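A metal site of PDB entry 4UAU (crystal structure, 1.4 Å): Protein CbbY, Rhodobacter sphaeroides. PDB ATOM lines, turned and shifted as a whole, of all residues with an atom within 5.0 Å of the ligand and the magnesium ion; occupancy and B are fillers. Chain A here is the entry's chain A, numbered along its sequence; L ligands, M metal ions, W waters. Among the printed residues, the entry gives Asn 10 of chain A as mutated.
OD2 of Asp 8 lies close to OG1 of Thr 12, at 2.8 Å. The side-chain amide nitrogen (ND2) of Asn 10 is in hydrogen-bond range of the side-chain hydroxyl (OG1) of Thr 117 (3.0 Å). OD1 of Asn 10 sits at hydrogen-bond distance from NE2 of His 20 (2.8 Å). OG1 of Thr 115 is in hydrogen-bond range of N of Thr 117, 3.1 Å away. The backbone carbonyl oxygen of His 75 lies within hydrogen-bond range of the side-chain hydroxyl of Thr 79, 3.0 Å away. A ring nitrogen (ND1) of His 20 lies within hydrogen-bond range of the side-chain amino group (NZ) of Lys 78. The side-chain hydroxyl (OG1) of Thr 117 sits at hydrogen-bond distance from the side-chain amide nitrogen (ND2) of Asn 121 (3.0 Å). The backbone carbonyl oxygen of Lys 151 lies within hydrogen-bond range of the side-chain hydroxyl of Thr 49, at 2.8 Å.
An oxygen (O8) of the ligand sits at hydrogen-bond distance from the backbone NH of Asn 10 (2.7 Å). ND2 of Asn 10 sits at hydrogen-bond distance from O1 of the ligand, at 2.9 Å. An oxygen (O8) of the ligand lies within hydrogen-bond range of the side-chain hydroxyl of Thr 115, 2.5 Å away. The side-chain carboxylate (OE2) of Glu 17 sits at hydrogen-bond distance from an oxygen (O4) of the ligand (2.6 Å). NE2 of His 75 lies within hydrogen-bond range of O10 of the ligand. The backbone NH (N) of Gly 51 sits at hydrogen-bond distance from an oxygen (O11) of the ligand, 2.7 Å away. An oxygen (O9) of the ligand is in hydrogen-bond range of the backbone NH (N) of Ser 118 (2.9 Å). O9 of the ligand is in hydrogen-bond range of OG of Ser 118, at 2.8 Å. The backbone NH (N) of Thr 116 sits at hydrogen-bond distance from an oxygen (O6) of the ligand (2.9 Å). The side-chain hydroxyl (OG1) of Thr 116 lies within hydrogen-bond range of an oxygen (O6) of the ligand (2.8 Å). N of Gly 50 sits at hydrogen-bond distance from O3 of the ligand. NZ of Lys 78 is in salt-bridge range of O10 of the ligand (2.8 Å). An oxygen (O4) of the ligand lies within hydrogen-bond range of the guanidinium group of Arg 54 (2.9 Å). OG1 of Thr 117 lies within hydrogen-bond range of O5 of the ligand, at 2.9 Å. O9 of the ligand is in hydrogen-bond range of ND2 of Asn 121 (3.1 Å). The backbone NH (N) of Val 9 lies within hydrogen-bond range of an oxygen (O8) of the ligand (3.4 Å). The side-chain amino group of Lys 151 is in salt-bridge range of an oxygen (O6) of the ligand, 3.5 Å away.
The magnesium ion is bound by O7 of the ligand (1.9 Å), OD2 of Asp 8 (2.0 Å), OD1 of Asp 176 (2.1 Å), water W5 (2.1 Å), water W3 (2.2 Å) and O of Asn 10 (2.2 Å).
Water W5 lies within hydrogen-bond range of OE1 of Glu 175, OG of Ser 177 and OD1 of Asp 8. Water W6 bridges an oxygen (O11) of the ligand and the backbone carbonyl oxygen (O) of Thr 116. Water W1 lies within hydrogen-bond range of O9 of the ligand (2.7 Å), NZ of Lys 78 (2.7 Å), OG1 of Thr 79 (2.8 Å), ND2 of Asn 121 (2.9 Å), OG of Ser 118 (3.4 Å) and NE2 of His 75 (3.5 Å). Water W2 bridges O of Leu 46 and O2 of the ligand.
Residues that only touch the ligand: Thr 49, His 20, Phe 24 and Leu 46. Hydrophobic or aromatic side chains within 4 Å of the ligand: Val 9, His 20, Phe 24, Leu 46 and His 75. Of the 27 residues printed, 19 come within 4 Å of the ligand. Along chain A the residues within 4 Å of the ligand span positions 8 to 151. The nearest printed residue that does not touch the ligand is Asp 176 (4.01 Å).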
ATOM      1  N   ASP A   8      -5.161   2.339  -9.788  1.00  0.00           N
ATOM      2  CA  ASP A   8      -4.714   0.970  -9.635  1.00  0.00           C
ATOM      3  C   ASP A   8      -3.366   0.779 -10.354  1.00  0.00           C
ATOM      4  O   ASP A   8      -2.982   1.603 -11.204  1.00  0.00           O
ATOM      5  CB  ASP A   8      -5.788   0.031 -10.200  1.00  0.00           C
ATOM      6  CG  ASP A   8      -5.393  -1.401 -10.103  1.00  0.00           C
ATOM      7  OD1 ASP A   8      -5.073  -1.814  -8.956  1.00  0.00           O
ATOM      8  OD2 ASP A   8      -5.364  -2.074 -11.139  1.00  0.00           O
ATOM      9  N   VAL A   9      -2.652  -0.303 -10.044  1.00  0.00           N
ATOM     10  CA  VAL A   9      -1.365  -0.565 -10.708  1.00  0.00           C
ATOM     11  C   VAL A   9      -1.485  -1.695 -11.734  1.00  0.00           C
ATOM     12  O   VAL A   9      -1.479  -1.433 -12.939  1.00  0.00           O
ATOM     13  CB  VAL A   9      -0.226  -0.853  -9.705  1.00  0.00           C
ATOM     14  CG1 VAL A   9       1.074  -1.299 -10.404  1.00  0.00           C
ATOM     15  CG2 VAL A   9       0.055   0.392  -8.895  1.00  0.00           C
ATOM     16  N   ASN A  10      -1.680  -2.939 -11.271  1.00  0.00           N
ATOM     17  CA  ASN A  10      -1.605  -4.073 -12.188  1.00  0.00           C
ATOM     18  C   ASN A  10      -2.786  -4.132 -13.122  1.00  0.00           C
ATOM     19  O   ASN A  10      -3.946  -4.183 -12.672  1.00  0.00           O
ATOM     20  CB  ASN A  10      -1.398  -5.366 -11.411  1.00  0.00           C
ATOM     21  CG  ASN A  10      -0.046  -5.391 -10.703  1.00  0.00           C
ATOM     22  OD1 ASN A  10       1.001  -5.209 -11.342  1.00  0.00           O
ATOM     23  ND2 ASN A  10      -0.065  -5.552  -9.395  1.00  0.00           N
ATOM     24  N   GLY A  11      -2.519  -4.087 -14.423  1.00  0.00           N
ATOM     25  CA  GLY A  11      -3.596  -4.074 -15.397  1.00  0.00           C
ATOM     26  C   GLY A  11      -4.111  -2.691 -15.730  1.00  0.00           C
ATOM     27  O   GLY A  11      -4.906  -2.542 -16.661  1.00  0.00           O
ATOM     28  N   THR A  12      -3.699  -1.685 -14.961  1.00  0.00           N
ATOM     29  CA  THR A  12      -4.211  -0.312 -15.117  1.00  0.00           C
ATOM     30  C   THR A  12      -3.110   0.621 -15.621  1.00  0.00           C
ATOM     31  O   THR A  12      -3.237   1.168 -16.732  1.00  0.00           O
ATOM     32  CB  THR A  12      -4.847   0.154 -13.794  1.00  0.00           C
ATOM     33  OG1 THR A  12      -5.976  -0.693 -13.498  1.00  0.00           O
ATOM     34  CG2 THR A  12      -5.340   1.544 -13.903  1.00  0.00           C
ATOM     35  N   GLU A  17       0.433  -8.672 -15.611  1.00  0.00           N
ATOM     36  CA  GLU A  17       0.159  -9.970 -14.958  1.00  0.00           C
ATOM     37  C   GLU A  17       0.905 -11.148 -15.554  1.00  0.00           C
ATOM     38  O   GLU A  17       1.239 -12.077 -14.837  1.00  0.00           O
ATOM     39  CB  GLU A  17      -1.346 -10.248 -14.829  1.00  0.00           C
ATOM     40  CG  GLU A  17      -1.985  -9.445 -13.689  1.00  0.00           C
ATOM     41  CD  GLU A  17      -1.459  -9.787 -12.289  1.00  0.00           C
ATOM     42  OE1 GLU A  17      -0.702 -10.784 -12.121  1.00  0.00           O
ATOM     43  OE2 GLU A  17      -1.824  -9.057 -11.351  1.00  0.00           O
ATOM     44  N   HIS A  20       4.071 -11.025 -13.690  1.00  0.00           N
ATOM     45  CA  HIS A  20       3.828 -11.619 -12.377  1.00  0.00           C
ATOM     46  C   HIS A  20       3.802 -13.140 -12.451  1.00  0.00           C
ATOM     47  O   HIS A  20       4.425 -13.810 -11.624  1.00  0.00           O
ATOM     48  CB  HIS A  20       2.542 -11.088 -11.698  1.00  0.00           C
ATOM     49  CG  HIS A  20       2.660  -9.684 -11.194  1.00  0.00           C
ATOM     50  ND1 HIS A  20       3.392  -9.349 -10.084  1.00  0.00           N
ATOM     51  CD2 HIS A  20       2.081  -8.533 -11.626  1.00  0.00           C
ATOM     52  CE1 HIS A  20       3.286  -8.063  -9.858  1.00  0.00           C
ATOM     53  NE2 HIS A  20       2.504  -7.540 -10.782  1.00  0.00           N
ATOM     54  N   PHE A  24       6.231 -15.753 -10.448  1.00  0.00           N
ATOM     55  CA  PHE A  24       5.738 -16.842  -9.584  1.00  0.00           C
ATOM     56  C   PHE A  24       6.354 -18.161 -10.039  1.00  0.00           C
ATOM     57  O   PHE A  24       6.963 -18.889  -9.239  1.00  0.00           O
ATOM     58  CB  PHE A  24       4.201 -16.958  -9.607  1.00  0.00           C
ATOM     59  CG  PHE A  24       3.475 -15.957  -8.715  1.00  0.00           C
ATOM     60  CD1 PHE A  24       3.526 -16.069  -7.330  1.00  0.00           C
ATOM     61  CD2 PHE A  24       2.700 -14.924  -9.287  1.00  0.00           C
ATOM     62  CE1 PHE A  24       2.843 -15.157  -6.517  1.00  0.00           C
ATOM     63  CE2 PHE A  24       2.006 -14.026  -8.461  1.00  0.00           C
ATOM     64  CZ  PHE A  24       2.098 -14.148  -7.076  1.00  0.00           C
ATOM     65  N   TYR A  42      -4.049 -19.315 -13.655  1.00  0.00           N
ATOM     66  CA  TYR A  42      -3.799 -17.968 -13.156  1.00  0.00           C
ATOM     67  C   TYR A  42      -5.028 -17.051 -13.246  1.00  0.00           C
ATOM     68  O   TYR A  42      -5.269 -16.263 -12.327  1.00  0.00           O
ATOM     69  CB  TYR A  42      -2.574 -17.365 -13.873  1.00  0.00           C
ATOM     70  CG  TYR A  42      -1.941 -16.257 -13.086  1.00  0.00           C
ATOM     71  CD1 TYR A  42      -1.456 -16.472 -11.793  1.00  0.00           C
ATOM     72  CD2 TYR A  42      -1.789 -14.983 -13.669  1.00  0.00           C
ATOM     73  CE1 TYR A  42      -0.838 -15.400 -11.064  1.00  0.00           C
ATOM     74  CE2 TYR A  42      -1.182 -13.953 -12.970  1.00  0.00           C
ATOM     75  CZ  TYR A  42      -0.737 -14.151 -11.669  1.00  0.00           C
ATOM     76  OH  TYR A  42      -0.128 -13.117 -10.987  1.00  0.00           O
ATOM     77  N   LEU A  46      -6.309 -15.138  -9.950  1.00  0.00           N
ATOM     78  CA  LEU A  46      -6.296 -13.671  -9.920  1.00  0.00           C
ATOM     79  C   LEU A  46      -7.514 -13.043  -9.241  1.00  0.00           C
ATOM     80  O   LEU A  46      -7.465 -11.862  -8.882  1.00  0.00           O
ATOM     81  CB  LEU A  46      -6.141 -13.111 -11.331  1.00  0.00           C
ATOM     82  CG  LEU A  46      -4.703 -13.079 -11.820  1.00  0.00           C
ATOM     83  CD1 LEU A  46      -4.694 -12.790 -13.335  1.00  0.00           C
ATOM     84  CD2 LEU A  46      -3.872 -12.029 -11.076  1.00  0.00           C
ATOM     85  N   THR A  48      -8.310 -13.710  -6.302  1.00  0.00           N
ATOM     86  CA  THR A  48      -7.803 -13.454  -4.953  1.00  0.00           C
ATOM     87  C   THR A  48      -6.659 -12.484  -5.079  1.00  0.00           C
ATOM     88  O   THR A  48      -5.669 -12.825  -5.725  1.00  0.00           O
ATOM     89  CB  THR A  48      -7.270 -14.757  -4.323  1.00  0.00           C
ATOM     90  OG1 THR A  48      -8.386 -15.639  -4.118  1.00  0.00           O
ATOM     91  CG2 THR A  48      -6.563 -14.488  -2.998  1.00  0.00           C
ATOM     92  N   THR A  49      -6.800 -11.273  -4.511  1.00  0.00           N
ATOM     93  CA  THR A  49      -5.726 -10.291  -4.645  1.00  0.00           C
ATOM     94  C   THR A  49      -4.651 -10.484  -3.551  1.00  0.00           C
ATOM     95  O   THR A  49      -4.933 -10.977  -2.430  1.00  0.00           O
ATOM     96  CB  THR A  49      -6.232  -8.830  -4.588  1.00  0.00           C
ATOM     97  OG1 THR A  49      -6.717  -8.522  -3.271  1.00  0.00           O
ATOM     98  CG2 THR A  49      -7.364  -8.633  -5.583  1.00  0.00           C
ATOM     99  N   GLY A  50      -3.432 -10.069  -3.891  1.00  0.00           N
ATOM    100  CA  GLY A  50      -2.257 -10.246  -3.025  1.00  0.00           C
ATOM    101  C   GLY A  50      -1.588 -11.582  -3.308  1.00  0.00           C
ATOM    102  O   GLY A  50      -2.206 -12.636  -3.268  1.00  0.00           O
ATOM    103  N   GLY A  51      -0.294 -11.540  -3.542  1.00  0.00           N
ATOM    104  CA  GLY A  51       0.410 -12.765  -3.895  1.00  0.00           C
ATOM    105  C   GLY A  51       0.500 -13.786  -2.782  1.00  0.00           C
ATOM    106  O   GLY A  51       0.463 -15.004  -3.036  1.00  0.00           O
ATOM    107  N   ARG A  54      -2.827 -15.392  -2.665  1.00  0.00           N
ATOM    108  CA  ARG A  54      -3.023 -16.247  -3.835  1.00  0.00           C
ATOM    109  C   ARG A  54      -2.303 -17.569  -3.657  1.00  0.00           C
ATOM    110  O   ARG A  54      -2.869 -18.628  -3.949  1.00  0.00           O
ATOM    111  CB  ARG A  54      -2.492 -15.545  -5.070  1.00  0.00           C
ATOM    112  CG  ARG A  54      -2.856 -16.251  -6.381  1.00  0.00           C
ATOM    113  CD  ARG A  54      -2.532 -15.387  -7.642  1.00  0.00           C
ATOM    114  NE  ARG A  54      -3.249 -14.131  -7.533  1.00  0.00           N
ATOM    115  CZ  ARG A  54      -2.759 -12.920  -7.727  1.00  0.00           C
ATOM    116  NH1 ARG A  54      -1.565 -12.731  -8.270  1.00  0.00           N
ATOM    117  NH2 ARG A  54      -3.539 -11.887  -7.398  1.00  0.00           N
ATOM    118  N   HIS A  75       6.899 -15.561  -1.244  1.00  0.00           N
ATOM    119  CA  HIS A  75       6.436 -14.354  -1.888  1.00  0.00           C
ATOM    120  C   HIS A  75       7.494 -13.260  -1.941  1.00  0.00           C
ATOM    121  O   HIS A  75       7.598 -12.512  -2.895  1.00  0.00           O
ATOM    122  CB  HIS A  75       5.184 -13.804  -1.243  1.00  0.00           C
ATOM    123  CG  HIS A  75       4.552 -12.731  -2.058  1.00  0.00           C
ATOM    124  ND1 HIS A  75       4.442 -11.426  -1.625  1.00  0.00           N
ATOM    125  CD2 HIS A  75       4.059 -12.751  -3.327  1.00  0.00           C
ATOM    126  CE1 HIS A  75       3.885 -10.699  -2.576  1.00  0.00           C
ATOM    127  NE2 HIS A  75       3.649 -11.474  -3.621  1.00  0.00           N
ATOM    128  N   LYS A  78       9.583 -14.105  -4.854  1.00  0.00           N
ATOM    129  CA  LYS A  78       8.840 -13.784  -6.066  1.00  0.00           C
ATOM    130  C   LYS A  78       8.880 -12.276  -6.335  1.00  0.00           C
ATOM    131  O   LYS A  78       9.050 -11.824  -7.492  1.00  0.00           O
ATOM    132  CB  LYS A  78       7.418 -14.318  -5.967  1.00  0.00           C
ATOM    133  CG  LYS A  78       6.516 -13.871  -7.146  1.00  0.00           C
ATOM    134  CD  LYS A  78       5.758 -12.572  -6.855  1.00  0.00           C
ATOM    135  CE  LYS A  78       5.115 -12.052  -8.104  1.00  0.00           C
ATOM    136  NZ  LYS A  78       4.367 -10.795  -7.781  1.00  0.00           N
ATOM    137  N   THR A  79       8.736 -11.478  -5.275  1.00  0.00           N
ATOM    138  CA  THR A  79       8.855 -10.027  -5.422  1.00  0.00           C
ATOM    139  C   THR A  79      10.230  -9.606  -5.941  1.00  0.00           C
ATOM    140  O   THR A  79      10.331  -8.809  -6.883  1.00  0.00           O
ATOM    141  CB  THR A  79       8.522  -9.309  -4.103  1.00  0.00           C
ATOM    142  OG1 THR A  79       7.189  -9.652  -3.734  1.00  0.00           O
ATOM    143  CG2 THR A  79       8.662  -7.803  -4.234  1.00  0.00           C
ATOM    144  N   THR A 115      -3.210   0.054  -4.568  1.00  0.00           N
ATOM    145  CA  THR A 115      -2.909  -1.248  -5.184  1.00  0.00           C
ATOM    146  C   THR A 115      -2.765  -2.318  -4.146  1.00  0.00           C
ATOM    147  O   THR A 115      -2.399  -2.044  -2.993  1.00  0.00           O
ATOM    148  CB  THR A 115      -1.619  -1.150  -6.049  1.00  0.00           C
ATOM    149  OG1 THR A 115      -1.360  -2.412  -6.664  1.00  0.00           O
ATOM    150  CG2 THR A 115      -0.410  -0.748  -5.218  1.00  0.00           C
ATOM    151  N   THR A 116      -3.066  -3.543  -4.551  1.00  0.00           N
ATOM    152  CA  THR A 116      -2.850  -4.739  -3.725  1.00  0.00           C
ATOM    153  C   THR A 116      -1.422  -5.244  -3.815  1.00  0.00           C
ATOM    154  O   THR A 116      -1.016  -6.082  -3.003  1.00  0.00           O
ATOM    155  CB  THR A 116      -3.800  -5.909  -4.114  1.00  0.00           C
ATOM    156  OG1 THR A 116      -3.504  -6.338  -5.452  1.00  0.00           O
ATOM    157  CG2 THR A 116      -5.278  -5.463  -4.031  1.00  0.00           C
ATOM    158  N   THR A 117      -0.665  -4.737  -4.791  1.00  0.00           N
ATOM    159  CA  THR A 117       0.686  -5.264  -5.083  1.00  0.00           C
ATOM    160  C   THR A 117       1.728  -4.794  -4.078  1.00  0.00           C
ATOM    161  O   THR A 117       1.545  -3.749  -3.406  1.00  0.00           O
ATOM    162  CB  THR A 117       1.071  -4.862  -6.554  1.00  0.00           C
ATOM    163  OG1 THR A 117       1.948  -5.838  -7.131  1.00  0.00           O
ATOM    164  CG2 THR A 117       1.765  -3.503  -6.660  1.00  0.00           C
ATOM    165  N   SER A 118       2.824  -5.543  -4.008  1.00  0.00           N
ATOM    166  CA  SER A 118       3.953  -5.200  -3.125  1.00  0.00           C
ATOM    167  C   SER A 118       4.570  -3.862  -3.499  1.00  0.00           C
ATOM    168  O   SER A 118       4.760  -3.566  -4.677  1.00  0.00           O
ATOM    169  CB  SER A 118       5.010  -6.287  -3.216  1.00  0.00           C
ATOM    170  OG  SER A 118       4.418  -7.524  -2.916  1.00  0.00           O
ATOM    171  N   ASN A 121       7.254  -3.387  -6.195  1.00  0.00           N
ATOM    172  CA  ASN A 121       6.779  -3.515  -7.563  1.00  0.00           C
ATOM    173  C   ASN A 121       6.372  -2.175  -8.157  1.00  0.00           C
ATOM    174  O   ASN A 121       6.513  -1.957  -9.352  1.00  0.00           O
ATOM    175  CB  ASN A 121       5.560  -4.441  -7.628  1.00  0.00           C
ATOM    176  CG  ASN A 121       5.877  -5.856  -7.191  1.00  0.00           C
ATOM    177  OD1 ASN A 121       7.042  -6.271  -7.132  1.00  0.00           O
ATOM    178  ND2 ASN A 121       4.827  -6.618  -6.927  1.00  0.00           N
ATOM    179  N   LYS A 151      -8.266  -5.498  -1.674  1.00  0.00           N
ATOM    180  CA  LYS A 151      -9.425  -5.376  -2.577  1.00  0.00           C
ATOM    181  C   LYS A 151     -10.045  -6.767  -2.719  1.00  0.00           C
ATOM    182  O   LYS A 151      -9.335  -7.758  -2.899  1.00  0.00           O
ATOM    183  CB  LYS A 151      -9.020  -4.803  -3.943  1.00  0.00           C
ATOM    184  CG  LYS A 151      -8.170  -3.517  -3.890  1.00  0.00           C
ATOM    185  CD  LYS A 151      -7.928  -2.959  -5.278  1.00  0.00           C
ATOM    186  CE  LYS A 151      -6.872  -1.899  -5.250  1.00  0.00           C
ATOM    187  NZ  LYS A 151      -6.454  -1.597  -6.673  1.00  0.00           N
ATOM    188  N   GLU A 175      -9.383   1.690 -12.725  1.00  0.00           N
ATOM    189  CA  GLU A 175      -9.259   0.257 -12.366  1.00  0.00           C
ATOM    190  C   GLU A 175      -9.371  -0.611 -13.593  1.00  0.00           C
ATOM    191  O   GLU A 175      -9.858  -0.162 -14.659  1.00  0.00           O
ATOM    192  CB  GLU A 175     -10.367  -0.131 -11.378  1.00  0.00           C
ATOM    193  CG  GLU A 175      -9.991   0.187  -9.950  1.00  0.00           C
ATOM    194  CD  GLU A 175      -9.027  -0.821  -9.371  1.00  0.00           C
ATOM    195  OE1 GLU A 175      -8.622  -1.763 -10.091  1.00  0.00           O
ATOM    196  OE2 GLU A 175      -8.618  -0.638  -8.191  1.00  0.00           O
ATOM    197  N   ASP A 176      -8.953  -1.860 -13.442  1.00  0.00           N
ATOM    198  CA  ASP A 176      -9.054  -2.855 -14.503  1.00  0.00           C
ATOM    199  C   ASP A 176      -9.842  -4.087 -14.156  1.00  0.00           C
ATOM    200  O   ASP A 176     -10.143  -4.884 -15.026  1.00  0.00           O
ATOM    201  CB  ASP A 176      -7.652  -3.323 -14.943  1.00  0.00           C
ATOM    202  CG  ASP A 176      -6.977  -4.188 -13.863  1.00  0.00           C
ATOM    203  OD1 ASP A 176      -6.818  -3.695 -12.717  1.00  0.00           O
ATOM    204  OD2 ASP A 176      -6.657  -5.376 -14.133  1.00  0.00           O
ATOM    205  N   SER A 177     -10.129  -4.272 -12.867  1.00  0.00           N
ATOM    206  CA  SER A 177     -10.703  -5.522 -12.391  1.00  0.00           C
ATOM    207  C   SER A 177     -11.962  -5.317 -11.542  1.00  0.00           C
ATOM    208  O   SER A 177     -12.195  -4.242 -11.003  1.00  0.00           O
ATOM    209  CB  SER A 177      -9.663  -6.332 -11.582  1.00  0.00           C
ATOM    210  OG  SER A 177      -9.419  -5.727 -10.323  1.00  0.00           O
HETATM  211  C1  LIG L   1      -3.405  -7.104  -8.459  1.00  0.00           C
HETATM  212  C2  LIG L   1      -3.024  -8.215  -7.486  1.00  0.00           C
HETATM  213  C3  LIG L   1      -1.618  -8.411  -7.015  1.00  0.00           C
HETATM  214  C4  LIG L   1      -0.787  -8.908  -8.207  1.00  0.00           C
HETATM  215  C5  LIG L   1       0.550  -9.504  -7.800  1.00  0.00           C
HETATM  216  O1  LIG L   1      -2.713  -5.832  -8.260  1.00  0.00           O
HETATM  217  O2  LIG L   1      -3.914  -9.009  -7.136  1.00  0.00           O
HETATM  218  O3  LIG L   1      -1.656  -9.363  -5.947  1.00  0.00           O
HETATM  219  O4  LIG L   1      -1.513  -9.948  -8.888  1.00  0.00           O
HETATM  220  O5  LIG L   1       1.305  -8.636  -6.959  1.00  0.00           O
HETATM  221  P1  LIG L   1      -3.503  -4.406  -8.458  1.00  0.00           P
HETATM  222  P2  LIG L   1       1.861  -9.181  -5.554  1.00  0.00           P
HETATM  223  O6  LIG L   1      -4.244  -4.250  -7.149  1.00  0.00           O
HETATM  224  O7  LIG L   1      -4.392  -4.615  -9.666  1.00  0.00           O
HETATM  225  O8  LIG L   1      -2.394  -3.405  -8.692  1.00  0.00           O
HETATM  226  O9  LIG L   1       2.911  -8.197  -5.152  1.00  0.00           O
HETATM  227  O10 LIG L   1       2.404 -10.583  -5.785  1.00  0.00           O
HETATM  228  O11 LIG L   1       0.716  -9.222  -4.581  1.00  0.00           O
HETATM  229 MG    MG M   1      -5.525  -4.082 -11.155  1.00  0.00          MG
HETATM  230  O   HOH W   1       5.319  -9.253  -5.714  1.00  0.00           O
HETATM  231  O   HOH W   2      -5.832  -9.599  -9.164  1.00  0.00           O
HETATM  232  O   HOH W   3      -5.939  -6.178 -11.612  1.00  0.00           O
HETATM  233  O   HOH W   4      -6.793  -5.199  -7.497  1.00  0.00           O
HETATM  234  O   HOH W   5      -7.284  -4.034  -9.939  1.00  0.00           O
HETATM  235  O   HOH W   6       0.599  -8.192  -2.176  1.00  0.00           O
